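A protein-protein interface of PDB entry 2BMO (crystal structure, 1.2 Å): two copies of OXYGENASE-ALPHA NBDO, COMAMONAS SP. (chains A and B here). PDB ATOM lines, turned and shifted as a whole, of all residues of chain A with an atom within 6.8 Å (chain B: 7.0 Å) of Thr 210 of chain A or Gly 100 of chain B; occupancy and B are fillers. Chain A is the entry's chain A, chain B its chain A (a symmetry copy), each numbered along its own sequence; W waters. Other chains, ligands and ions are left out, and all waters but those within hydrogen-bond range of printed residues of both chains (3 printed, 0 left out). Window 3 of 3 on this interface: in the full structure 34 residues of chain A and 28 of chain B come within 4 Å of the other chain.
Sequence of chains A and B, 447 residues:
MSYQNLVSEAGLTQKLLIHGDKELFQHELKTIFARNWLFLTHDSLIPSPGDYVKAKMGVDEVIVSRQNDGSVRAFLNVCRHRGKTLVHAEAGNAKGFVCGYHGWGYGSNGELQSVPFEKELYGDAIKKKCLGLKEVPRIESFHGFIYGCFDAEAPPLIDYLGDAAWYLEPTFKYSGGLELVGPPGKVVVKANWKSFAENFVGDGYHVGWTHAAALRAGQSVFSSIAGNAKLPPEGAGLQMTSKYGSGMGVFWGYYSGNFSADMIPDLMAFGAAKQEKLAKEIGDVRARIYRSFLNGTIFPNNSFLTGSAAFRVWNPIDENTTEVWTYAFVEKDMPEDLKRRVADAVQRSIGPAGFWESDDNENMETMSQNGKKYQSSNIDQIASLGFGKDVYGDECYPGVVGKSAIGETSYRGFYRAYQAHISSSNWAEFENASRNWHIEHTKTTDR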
ATOM      1  N   ASN A 199     -13.466  23.282 -12.935  1.00  0.00           N
ATOM      2  CA  ASN A 199     -13.374  21.882 -12.546  1.00  0.00           C
ATOM      3  C   ASN A 199     -14.549  21.492 -11.647  1.00  0.00           C
ATOM      4  O   ASN A 199     -15.186  20.455 -11.845  1.00  0.00           O
ATOM      5  CB  ASN A 199     -12.036  21.610 -11.867  1.00  0.00           C
ATOM      6  CG  ASN A 199     -11.835  20.150 -11.534  1.00  0.00           C
ATOM      7  OD1 ASN A 199     -11.951  19.760 -10.384  1.00  0.00           O
ATOM      8  ND2 ASN A 199     -11.543  19.333 -12.542  1.00  0.00           N
ATOM      9  N   ASP A 203     -17.036  19.261 -13.901  1.00  0.00           N
ATOM     10  CA  ASP A 203     -16.106  18.238 -14.399  1.00  0.00           C
ATOM     11  C   ASP A 203     -16.347  16.841 -13.805  1.00  0.00           C
ATOM     12  O   ASP A 203     -15.600  16.395 -12.932  1.00  0.00           O
ATOM     13  CB  ASP A 203     -14.643  18.667 -14.244  1.00  0.00           C
ATOM     14  CG  ASP A 203     -13.729  17.918 -15.183  1.00  0.00           C
ATOM     15  OD1 ASP A 203     -12.627  18.417 -15.461  1.00  0.00           O
ATOM     16  OD2 ASP A 203     -14.123  16.832 -15.648  1.00  0.00           O
ATOM     17  N   TYR A 205     -16.277  14.398 -16.001  1.00  0.00           N
ATOM     18  CA  TYR A 205     -15.445  13.686 -16.972  1.00  0.00           C
ATOM     19  C   TYR A 205     -14.061  13.308 -16.433  1.00  0.00           C
ATOM     20  O   TYR A 205     -13.530  12.252 -16.781  1.00  0.00           O
ATOM     21  CB  TYR A 205     -15.307  14.576 -18.205  1.00  0.00           C
ATOM     22  CG  TYR A 205     -14.793  13.971 -19.508  1.00  0.00           C
ATOM     23  CD1 TYR A 205     -14.794  12.595 -19.762  1.00  0.00           C
ATOM     24  CD2 TYR A 205     -14.360  14.819 -20.518  1.00  0.00           C
ATOM     25  CE1 TYR A 205     -14.329  12.092 -20.997  1.00  0.00           C
ATOM     26  CE2 TYR A 205     -13.917  14.339 -21.740  1.00  0.00           C
ATOM     27  CZ  TYR A 205     -13.901  12.990 -21.974  1.00  0.00           C
ATOM     28  OH  TYR A 205     -13.456  12.559 -23.206  1.00  0.00           O
ATOM     29  N   HIS A 206     -13.482  14.138 -15.569  1.00  0.00           N
ATOM     30  CA  HIS A 206     -12.108  13.871 -15.106  1.00  0.00           C
ATOM     31  C   HIS A 206     -12.020  12.746 -14.088  1.00  0.00           C
ATOM     32  O   HIS A 206     -10.961  12.139 -13.929  1.00  0.00           O
ATOM     33  CB  HIS A 206     -11.435  15.133 -14.536  1.00  0.00           C
ATOM     34  CG  HIS A 206     -11.743  15.401 -13.088  1.00  0.00           C
ATOM     35  ND1 HIS A 206     -12.968  15.867 -12.659  1.00  0.00           N
ATOM     36  CD2 HIS A 206     -10.981  15.291 -11.973  1.00  0.00           C
ATOM     37  CE1 HIS A 206     -12.951  16.021 -11.347  1.00  0.00           C
ATOM     38  NE2 HIS A 206     -11.754  15.687 -10.904  1.00  0.00           N
ATOM     39  N   VAL A 207     -13.114  12.485 -13.380  1.00  0.00           N
ATOM     40  CA  VAL A 207     -13.047  11.667 -12.169  1.00  0.00           C
ATOM     41  C   VAL A 207     -12.404  10.305 -12.413  1.00  0.00           C
ATOM     42  O   VAL A 207     -11.455   9.928 -11.727  1.00  0.00           O
ATOM     43  CB  VAL A 207     -14.431  11.517 -11.495  1.00  0.00           C
ATOM     44  CG1 VAL A 207     -14.343  10.595 -10.283  1.00  0.00           C
ATOM     45  CG2 VAL A 207     -14.977  12.885 -11.087  1.00  0.00           C
ATOM     46  N   GLY A 208     -12.901   9.587 -13.415  1.00  0.00           N
ATOM     47  CA  GLY A 208     -12.433   8.236 -13.676  1.00  0.00           C
ATOM     48  C   GLY A 208     -11.013   8.140 -14.196  1.00  0.00           C
ATOM     49  O   GLY A 208     -10.396   7.079 -14.122  1.00  0.00           O
ATOM     50  N   TRP A 209     -10.493   9.246 -14.717  1.00  0.00           N
ATOM     51  CA  TRP A 209      -9.150   9.263 -15.299  1.00  0.00           C
ATOM     52  C   TRP A 209      -8.131   9.887 -14.347  1.00  0.00           C
ATOM     53  O   TRP A 209      -7.179   9.230 -13.918  1.00  0.00           O
ATOM     54  CB  TRP A 209      -9.140   9.993 -16.643  1.00  0.00           C
ATOM     55  CG  TRP A 209      -7.988   9.560 -17.471  1.00  0.00           C
ATOM     56  CD1 TRP A 209      -6.704  10.033 -17.426  1.00  0.00           C
ATOM     57  CD2 TRP A 209      -8.002   8.529 -18.454  1.00  0.00           C
ATOM     58  NE1 TRP A 209      -5.919   9.354 -18.323  1.00  0.00           N
ATOM     59  CE2 TRP A 209      -6.695   8.428 -18.974  1.00  0.00           C
ATOM     60  CE3 TRP A 209      -9.002   7.686 -18.958  1.00  0.00           C
ATOM     61  CZ2 TRP A 209      -6.362   7.521 -19.986  1.00  0.00           C
ATOM     62  CZ3 TRP A 209      -8.671   6.783 -19.959  1.00  0.00           C
ATOM     63  CH2 TRP A 209      -7.362   6.708 -20.462  1.00  0.00           C
ATOM     64  N   THR A 210      -8.336  11.162 -14.036  1.00  0.00           N
ATOM     65  CA  THR A 210      -7.479  11.873 -13.096  1.00  0.00           C
ATOM     66  C   THR A 210      -7.333  11.101 -11.781  1.00  0.00           C
ATOM     67  O   THR A 210      -6.231  11.004 -11.236  1.00  0.00           O
ATOM     68  CB  THR A 210      -8.057  13.273 -12.815  1.00  0.00           C
ATOM     69  OG1 THR A 210      -7.832  14.132 -13.932  1.00  0.00           O
ATOM     70  CG2 THR A 210      -7.447  13.902 -11.586  1.00  0.00           C
ATOM     71  N   HIS A 211      -8.442  10.556 -11.272  1.00  0.00           N
ATOM     72  CA  HIS A 211      -8.458   9.915  -9.960  1.00  0.00           C
ATOM     73  C   HIS A 211      -8.420   8.395 -10.003  1.00  0.00           C
ATOM     74  O   HIS A 211      -8.744   7.745  -9.005  1.00  0.00           O
ATOM     75  CB  HIS A 211      -9.659  10.398  -9.136  1.00  0.00           C
ATOM     76  CG  HIS A 211      -9.683  11.879  -8.924  1.00  0.00           C
ATOM     77  ND1 HIS A 211      -8.709  12.550  -8.214  1.00  0.00           N
ATOM     78  CD2 HIS A 211     -10.583  12.818  -9.305  1.00  0.00           C
ATOM     79  CE1 HIS A 211      -9.001  13.841  -8.184  1.00  0.00           C
ATOM     80  NE2 HIS A 211     -10.127  14.032  -8.848  1.00  0.00           N
ATOM     81  N   ALA A 212      -7.973   7.824 -11.124  1.00  0.00           N
ATOM     82  CA  ALA A 212      -7.924   6.364 -11.239  1.00  0.00           C
ATOM     83  C   ALA A 212      -7.216   5.680 -10.052  1.00  0.00           C
ATOM     84  O   ALA A 212      -7.720   4.691  -9.498  1.00  0.00           O
ATOM     85  CB  ALA A 212      -7.277   5.965 -12.556  1.00  0.00           C
ATOM     86  N   ALA A 213      -6.056   6.205  -9.662  1.00  0.00           N
ATOM     87  CA  ALA A 213      -5.300   5.610  -8.556  1.00  0.00           C
ATOM     88  C   ALA A 213      -6.048   5.737  -7.225  1.00  0.00           C
ATOM     89  O   ALA A 213      -6.100   4.799  -6.429  1.00  0.00           O
ATOM     90  CB  ALA A 213      -3.924   6.243  -8.457  1.00  0.00           C
ATOM     91  N   ALA A 214      -6.631   6.909  -6.994  1.00  0.00           N
ATOM     92  CA  ALA A 214      -7.378   7.177  -5.764  1.00  0.00           C
ATOM     93  C   ALA A 214      -8.599   6.268  -5.649  1.00  0.00           C
ATOM     94  O   ALA A 214      -8.947   5.807  -4.556  1.00  0.00           O
ATOM     95  CB  ALA A 214      -7.798   8.645  -5.710  1.00  0.00           C
ATOM     96  N   ASN A 228     -12.757   5.970 -17.220  1.00  0.00           N
ATOM     97  CA  ASN A 228     -13.761   6.482 -18.164  1.00  0.00           C
ATOM     98  C   ASN A 228     -14.241   5.402 -19.131  1.00  0.00           C
ATOM     99  O   ASN A 228     -14.485   5.666 -20.308  1.00  0.00           O
ATOM    100  CB  ASN A 228     -13.245   7.726 -18.901  1.00  0.00           C
ATOM    101  CG  ASN A 228     -13.265   8.961 -18.021  1.00  0.00           C
ATOM    102  OD1 ASN A 228     -13.939   8.978 -16.993  1.00  0.00           O
ATOM    103  ND2 ASN A 228     -12.530   9.995 -18.412  1.00  0.00           N
ATOM    104  N   TRP A 356      -6.833  13.060  -3.235  1.00  0.00           N
ATOM    105  CA  TRP A 356      -7.513  13.426  -4.484  1.00  0.00           C
ATOM    106  C   TRP A 356      -7.091  14.813  -4.950  1.00  0.00           C
ATOM    107  O   TRP A 356      -6.870  15.023  -6.137  1.00  0.00           O
ATOM    108  CB  TRP A 356      -9.026  13.413  -4.327  1.00  0.00           C
ATOM    109  CG  TRP A 356      -9.655  12.080  -4.095  1.00  0.00           C
ATOM    110  CD1 TRP A 356      -9.373  11.189  -3.105  1.00  0.00           C
ATOM    111  CD2 TRP A 356     -10.736  11.522  -4.844  1.00  0.00           C
ATOM    112  NE1 TRP A 356     -10.193  10.086  -3.204  1.00  0.00           N
ATOM    113  CE2 TRP A 356     -11.051  10.278  -4.255  1.00  0.00           C
ATOM    114  CE3 TRP A 356     -11.480  11.960  -5.955  1.00  0.00           C
ATOM    115  CZ2 TRP A 356     -12.073   9.455  -4.746  1.00  0.00           C
ATOM    116  CZ3 TRP A 356     -12.494  11.143  -6.439  1.00  0.00           C
ATOM    117  CH2 TRP A 356     -12.776   9.906  -5.833  1.00  0.00           C
ATOM    118  N   SER A 358      -4.302  16.301  -4.652  1.00  0.00           N
ATOM    119  CA  SER A 358      -3.032  16.170  -5.354  1.00  0.00           C
ATOM    120  C   SER A 358      -3.265  15.892  -6.846  1.00  0.00           C
ATOM    121  O   SER A 358      -2.617  16.490  -7.708  1.00  0.00           O
ATOM    122  CB  SER A 358      -2.198  15.057  -4.721  1.00  0.00           C
ATOM    123  OG  SER A 358      -1.005  14.819  -5.452  1.00  0.00           O
ATOM    124  N   ASP A 359      -4.196  14.989  -7.147  1.00  0.00           N
ATOM    125  CA  ASP A 359      -4.522  14.670  -8.542  1.00  0.00           C
ATOM    126  C   ASP A 359      -5.125  15.886  -9.252  1.00  0.00           C
ATOM    127  O   ASP A 359      -4.764  16.172 -10.393  1.00  0.00           O
ATOM    128  CB  ASP A 359      -5.544  13.538  -8.665  1.00  0.00           C
ATOM    129  CG  ASP A 359      -5.185  12.274  -7.904  1.00  0.00           C
ATOM    130  OD1 ASP A 359      -6.150  11.599  -7.500  1.00  0.00           O
ATOM    131  OD2 ASP A 359      -3.997  11.936  -7.733  1.00  0.00           O
ATOM    132  N   ASP A 360      -6.074  16.569  -8.604  1.00  0.00           N
ATOM    133  CA  ASP A 360      -6.755  17.715  -9.229  1.00  0.00           C
ATOM    134  C   ASP A 360      -5.781  18.865  -9.512  1.00  0.00           C
ATOM    135  O   ASP A 360      -5.813  19.463 -10.589  1.00  0.00           O
ATOM    136  CB  ASP A 360      -7.944  18.228  -8.388  1.00  0.00           C
ATOM    137  CG  ASP A 360      -9.122  17.257  -8.345  1.00  0.00           C
ATOM    138  OD1 ASP A 360      -9.703  16.872  -9.383  1.00  0.00           O
ATOM    139  OD2 ASP A 360      -9.529  16.895  -7.229  1.00  0.00           O
ATOM    140  N   ASN A 361      -4.921  19.170  -8.537  1.00  0.00           N
ATOM    141  CA  ASN A 361      -3.953  20.267  -8.656  1.00  0.00           C
ATOM    142  C   ASN A 361      -2.960  20.059  -9.783  1.00  0.00           C
ATOM    143  O   ASN A 361      -2.471  21.014 -10.392  1.00  0.00           O
ATOM    144  CB  ASN A 361      -3.188  20.449  -7.345  1.00  0.00           C
ATOM    145  CG  ASN A 361      -4.021  21.088  -6.261  1.00  0.00           C
ATOM    146  OD1 ASN A 361      -5.188  21.425  -6.462  1.00  0.00           O
ATOM    147  ND2 ASN A 361      -3.420  21.260  -5.094  1.00  0.00           N
ATOM    148  N   GLU A 362      -2.669  18.793 -10.055  1.00  0.00           N
ATOM    149  CA  GLU A 362      -1.815  18.424 -11.152  1.00  0.00           C
ATOM    150  C   GLU A 362      -2.394  18.991 -12.471  1.00  0.00           C
ATOM    151  O   GLU A 362      -1.664  19.497 -13.310  1.00  0.00           O
ATOM    152  CB  GLU A 362      -1.675  16.902 -11.150  1.00  0.00           C
ATOM    153  CG  GLU A 362      -1.096  16.295 -12.390  1.00  0.00           C
ATOM    154  CD  GLU A 362       0.370  16.602 -12.602  1.00  0.00           C
ATOM    155  OE1 GLU A 362       0.847  16.296 -13.712  1.00  0.00           O
ATOM    156  OE2 GLU A 362       1.035  17.137 -11.681  1.00  0.00           O
ATOM    157  N   ASN A 363      -3.718  18.965 -12.604  1.00  0.00           N
ATOM    158  CA  ASN A 363      -4.414  19.565 -13.750  1.00  0.00           C
ATOM    159  C   ASN A 363      -4.501  21.095 -13.723  1.00  0.00           C
ATOM    160  O   ASN A 363      -4.264  21.760 -14.725  1.00  0.00           O
ATOM    161  CB  ASN A 363      -5.816  18.971 -13.846  1.00  0.00           C
ATOM    162  CG  ASN A 363      -5.784  17.477 -14.030  1.00  0.00           C
ATOM    163  OD1 ASN A 363      -4.927  16.955 -14.744  1.00  0.00           O
ATOM    164  ND2 ASN A 363      -6.703  16.774 -13.382  1.00  0.00           N
ATOM    165  N   LYS B  84      -4.371  21.462 -20.578  1.00  0.00           N
ATOM    166  CA  LYS B  84      -3.372  20.865 -19.697  1.00  0.00           C
ATOM    167  C   LYS B  84      -2.076  20.542 -20.457  1.00  0.00           C
ATOM    168  O   LYS B  84      -2.103  20.171 -21.631  1.00  0.00           O
ATOM    169  CB  LYS B  84      -3.916  19.584 -19.060  1.00  0.00           C
ATOM    170  CG  LYS B  84      -3.147  19.135 -17.816  1.00  0.00           C
ATOM    171  CD  LYS B  84      -3.269  17.645 -17.584  1.00  0.00           C
ATOM    172  CE  LYS B  84      -2.258  17.173 -16.560  1.00  0.00           C
ATOM    173  NZ  LYS B  84      -0.946  16.857 -17.193  1.00  0.00           N
ATOM    174  N   THR B  85      -0.936  20.678 -19.785  1.00  0.00           N
ATOM    175  CA  THR B  85       0.334  20.215 -20.346  1.00  0.00           C
ATOM    176  C   THR B  85       0.266  18.710 -20.549  1.00  0.00           C
ATOM    177  O   THR B  85      -0.152  17.973 -19.655  1.00  0.00           O
ATOM    178  CB  THR B  85       1.474  20.601 -19.407  1.00  0.00           C
ATOM    179  OG1 THR B  85       1.567  22.029 -19.375  1.00  0.00           O
ATOM    180  CG2 THR B  85       2.805  20.010 -19.862  1.00  0.00           C
ATOM    181  N   LEU B  86       0.717  18.265 -21.716  1.00  0.00           N
ATOM    182  CA  LEU B  86       0.546  16.887 -22.111  1.00  0.00           C
ATOM    183  C   LEU B  86       1.661  15.952 -21.617  1.00  0.00           C
ATOM    184  O   LEU B  86       1.380  14.865 -21.107  1.00  0.00           O
ATOM    185  CB  LEU B  86       0.376  16.826 -23.630  1.00  0.00           C
ATOM    186  CG  LEU B  86       0.044  15.498 -24.292  1.00  0.00           C
ATOM    187  CD1 LEU B  86      -1.335  15.001 -23.894  1.00  0.00           C
ATOM    188  CD2 LEU B  86       0.105  15.688 -25.786  1.00  0.00           C
ATOM    189  N   VAL B  98      -0.961  10.491 -23.946  1.00  0.00           N
ATOM    190  CA  VAL B  98      -2.283  10.550 -23.333  1.00  0.00           C
ATOM    191  C   VAL B  98      -2.323  11.673 -22.295  1.00  0.00           C
ATOM    192  O   VAL B  98      -1.414  11.811 -21.458  1.00  0.00           O
ATOM    193  CB  VAL B  98      -2.664   9.188 -22.687  1.00  0.00           C
ATOM    194  CG1 VAL B  98      -4.051   9.243 -22.035  1.00  0.00           C
ATOM    195  CG2 VAL B  98      -2.611   8.066 -23.724  1.00  0.00           C
ATOM    196  N   CYS B  99      -3.375  12.482 -22.355  1.00  0.00           N
ATOM    197  CA  CYS B  99      -3.574  13.555 -21.398  1.00  0.00           C
ATOM    198  C   CYS B  99      -4.108  13.008 -20.080  1.00  0.00           C
ATOM    199  O   CYS B  99      -5.110  12.293 -20.054  1.00  0.00           O
ATOM    200  CB  CYS B  99      -4.534  14.590 -21.966  1.00  0.00           C
ATOM    201  SG  CYS B  99      -4.733  15.989 -20.841  1.00  0.00           S
ATOM    202  N   GLY B 100      -3.439  13.351 -18.985  1.00  0.00           N
ATOM    203  CA  GLY B 100      -3.823  12.850 -17.675  1.00  0.00           C
ATOM    204  C   GLY B 100      -5.082  13.445 -17.076  1.00  0.00           C
ATOM    205  O   GLY B 100      -5.522  12.986 -16.035  1.00  0.00           O
ATOM    206  N   TYR B 101      -5.668  14.461 -17.706  1.00  0.00           N
ATOM    207  CA  TYR B 101      -6.844  15.105 -17.128  1.00  0.00           C
ATOM    208  C   TYR B 101      -8.093  14.254 -17.417  1.00  0.00           C
ATOM    209  O   TYR B 101      -8.695  13.699 -16.486  1.00  0.00           O
ATOM    210  CB  TYR B 101      -6.942  16.536 -17.659  1.00  0.00           C
ATOM    211  CG  TYR B 101      -7.831  17.506 -16.886  1.00  0.00           C
ATOM    212  CD1 TYR B 101      -7.790  18.865 -17.186  1.00  0.00           C
ATOM    213  CD2 TYR B 101      -8.706  17.079 -15.878  1.00  0.00           C
ATOM    214  CE1 TYR B 101      -8.606  19.787 -16.510  1.00  0.00           C
ATOM    215  CE2 TYR B 101      -9.523  17.996 -15.195  1.00  0.00           C
ATOM    216  CZ  TYR B 101      -9.467  19.340 -15.518  1.00  0.00           C
ATOM    217  OH  TYR B 101     -10.268  20.253 -14.862  1.00  0.00           O
ATOM    218  N   HIS B 102      -8.462  14.129 -18.696  1.00  0.00           N
ATOM    219  CA  HIS B 102      -9.657  13.355 -19.082  1.00  0.00           C
ATOM    220  C   HIS B 102      -9.364  12.131 -19.938  1.00  0.00           C
ATOM    221  O   HIS B 102     -10.262  11.330 -20.191  1.00  0.00           O
ATOM    222  CB  HIS B 102     -10.711  14.230 -19.765  1.00  0.00           C
ATOM    223  CG  HIS B 102     -10.986  15.501 -19.034  1.00  0.00           C
ATOM    224  ND1 HIS B 102     -10.284  16.662 -19.280  1.00  0.00           N
ATOM    225  CD2 HIS B 102     -11.862  15.786 -18.037  1.00  0.00           C
ATOM    226  CE1 HIS B 102     -10.733  17.613 -18.475  1.00  0.00           C
ATOM    227  NE2 HIS B 102     -11.682  17.105 -17.705  1.00  0.00           N
ATOM    228  N   GLY B 103      -8.113  11.984 -20.373  1.00  0.00           N
ATOM    229  CA  GLY B 103      -7.700  10.783 -21.083  1.00  0.00           C
ATOM    230  C   GLY B 103      -7.680  10.846 -22.589  1.00  0.00           C
ATOM    231  O   GLY B 103      -7.578   9.800 -23.226  1.00  0.00           O
ATOM    232  N   TRP B 104      -7.752  12.041 -23.168  1.00  0.00           N
ATOM    233  CA  TRP B 104      -7.604  12.159 -24.628  1.00  0.00           C
ATOM    234  C   TRP B 104      -6.233  11.629 -25.037  1.00  0.00           C
ATOM    235  O   TRP B 104      -5.220  11.954 -24.402  1.00  0.00           O
ATOM    236  CB  TRP B 104      -7.749  13.602 -25.083  1.00  0.00           C
ATOM    237  CG  TRP B 104      -9.162  14.122 -25.102  1.00  0.00           C
ATOM    238  CD1 TRP B 104     -10.237  13.643 -24.393  1.00  0.00           C
ATOM    239  CD2 TRP B 104      -9.638  15.252 -25.830  1.00  0.00           C
ATOM    240  NE1 TRP B 104     -11.353  14.402 -24.661  1.00  0.00           N
ATOM    241  CE2 TRP B 104     -11.014  15.393 -25.541  1.00  0.00           C
ATOM    242  CE3 TRP B 104      -9.038  16.150 -26.725  1.00  0.00           C
ATOM    243  CZ2 TRP B 104     -11.794  16.403 -26.099  1.00  0.00           C
ATOM    244  CZ3 TRP B 104      -9.817  17.161 -27.281  1.00  0.00           C
ATOM    245  CH2 TRP B 104     -11.182  17.277 -26.962  1.00  0.00           C
HETATM  246  O   HOH W   1      -1.087  14.752 -15.326  1.00  0.00           O
HETATM  247  O   HOH W   2     -11.963  21.187 -16.826  1.00  0.00           O
HETATM  248  O   HOH W   3      -3.772  14.560 -14.426  1.00  0.00           O
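Of the printed residues of chain B, Thr 210 of chain A touches Gly 100 (3.3 Å) and Tyr 101 (2.7 Å).
Gly 100 of chain B touches just these residues of chain A: Trp 209 and Thr 210.
Of the printed residues of chain B, Asp 203 of chain A touches Tyr 101 (3.0 Å) and His 102 (2.8 Å).
Printed residues of chain B within 4 Å of Asn 199 of chain A: Tyr 101.
Of the printed residues of chain B, Glu 362 of chain A touches Lys 84.
Printed residues of chain A within 4 Å of Gly 103 of chain B: Trp 209.
Asp 359 of chain A touches none of the printed residues of chain B.
The nearest residue of chain B that does not touch Thr 210 of chain A is His 102 of chain B (4.8 Å).
No position is printed for both chains.
The side-chain amide nitrogen (ND2) of Asn 199 of chain A lies within hydrogen-bond range of the side-chain carboxylate (OD1) of Asp 203 of chain A, 3.2 Å away.
N of Tyr 205 of chain A is in hydrogen-bond range of OD2 of Asp 203 of chain A (3.3 Å).
ND1 of His 206 of chain A sits at hydrogen-bond distance from O of Asp 203 of chain A (2.7 Å).
The side-chain amide nitrogen (ND2) of Asn 363 of chain A sits at hydrogen-bond distance from the side-chain hydroxyl (OG1) of Thr 210 of chain A, at 2.9 Å.
The side-chain sulfur of Cys 99 of chain B sits close to the backbone NH of Tyr 101 of chain B (3.6 Å).
N of Cys 99 of chain B is in hydrogen-bond range of O of Trp 104 of chain B (2.8 Å).
Of the 20 printed residues of chain A, 9 touch a printed residue of chain B.
Printed residues of chain A that touch a printed residue of chain B: Asn 199, Asp 203, Tyr 205, His 206, Trp 209, Thr 210, Asn 228, Glu 362 and Asn 363.
Hydrophobic or aromatic side chains of chain A that line the printed part of chain B: Tyr 205, His 206 and Trp 209.
Hydrophobic or aromatic side chains of chain B within 4 Å of the printed part of chain A: Val 98, Tyr 101, His 102 and Trp 104.
Among the printed residues, 19 pairs touch across the chains.
Among the printed residues, Asp or Glu carboxylates within 4 Å of a Lys or Arg side-chain nitrogen of the other chain: Glu 362 of chain A with Lys 84 of chain B (3.96 Å).
The side-chain amide nitrogen of Asn 199 of chain A sits at hydrogen-bond distance from the side-chain hydroxyl of Tyr 101 of chain B (2.8 Å).
OH of Tyr 101 of chain B is in hydrogen-bond range of OD1 of Asp 203 of chain A, 3.0 Å away.
The side-chain carboxylate (OD1) of Asp 203 of chain A sits at hydrogen-bond distance from a ring nitrogen (NE2) of His 102 of chain B, at 2.8 Å.
The side-chain hydroxyl of Tyr 205 of chain A sits at hydrogen-bond distance from the indole nitrogen of Trp 104 of chain B, at 3.2 Å.
The backbone carbonyl oxygen of Gly 100 of chain B is in hydrogen-bond range of the side-chain hydroxyl of Thr 210 of chain A (3.3 Å).
OG1 of Thr 210 of chain A sits at hydrogen-bond distance from O of Tyr 101 of chain B, 2.7 Å away.
The side-chain amide nitrogen (ND2) of Asn 228 of chain A lies within hydrogen-bond range of the backbone carbonyl oxygen (O) of His 102 of chain B (3.2 Å).
The side-chain carboxylate (OE1) of Glu 362 of chain A lies within salt-bridge range of the side-chain amino group (NZ) of Lys 84 of chain B, 3.96 Å away.
Water W3 lies within hydrogen-bond range of OD1 of Asn 363 of chain A (2.7 Å) and O of Gly 100 of chain B (2.9 Å).
Water W2 lies within hydrogen-bond range of the side-chain hydroxyl (OH) of Tyr 101 of chain B (2.8 Å) and the side-chain carboxylate (OD1) of Asp 203 of chain A (3.2 Å).
Water W1 lies within hydrogen-bond range of the side-chain amino group (NZ) of Lys 84 of chain B (2.8 Å) and the side-chain carboxylate (OE1) of Glu 362 of chain A (3.0 Å).
Among the printed residues, merely in contact across the chains: Asn 363 of chain A with Tyr 101 of chain B (3.2 Å), Asn 363 of chain A with Lys 84 of chain B (3.2 Å), Trp 209 of chain A with Gly 103 of chain B (3.3 Å), His 206 of chain A with His 102 of chain B (3.4 Å), Trp 209 of chain A with Gly 100 of chain B (3.5 Å), His 206 of chain A with Tyr 101 of chain B (3.5 Å), Trp 209 of chain A with Cys 99 of chain B (3.5 Å), Trp 209 of chain A with Val 98 of chain B (3.5 Å), Tyr 205 of chain A with His 102 of chain B (3.7 Å), Trp 209 of chain A with Tyr 101 of chain B (3.7 Å) and Trp 209 of chain A with His 102 of chain B (3.8 Å).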
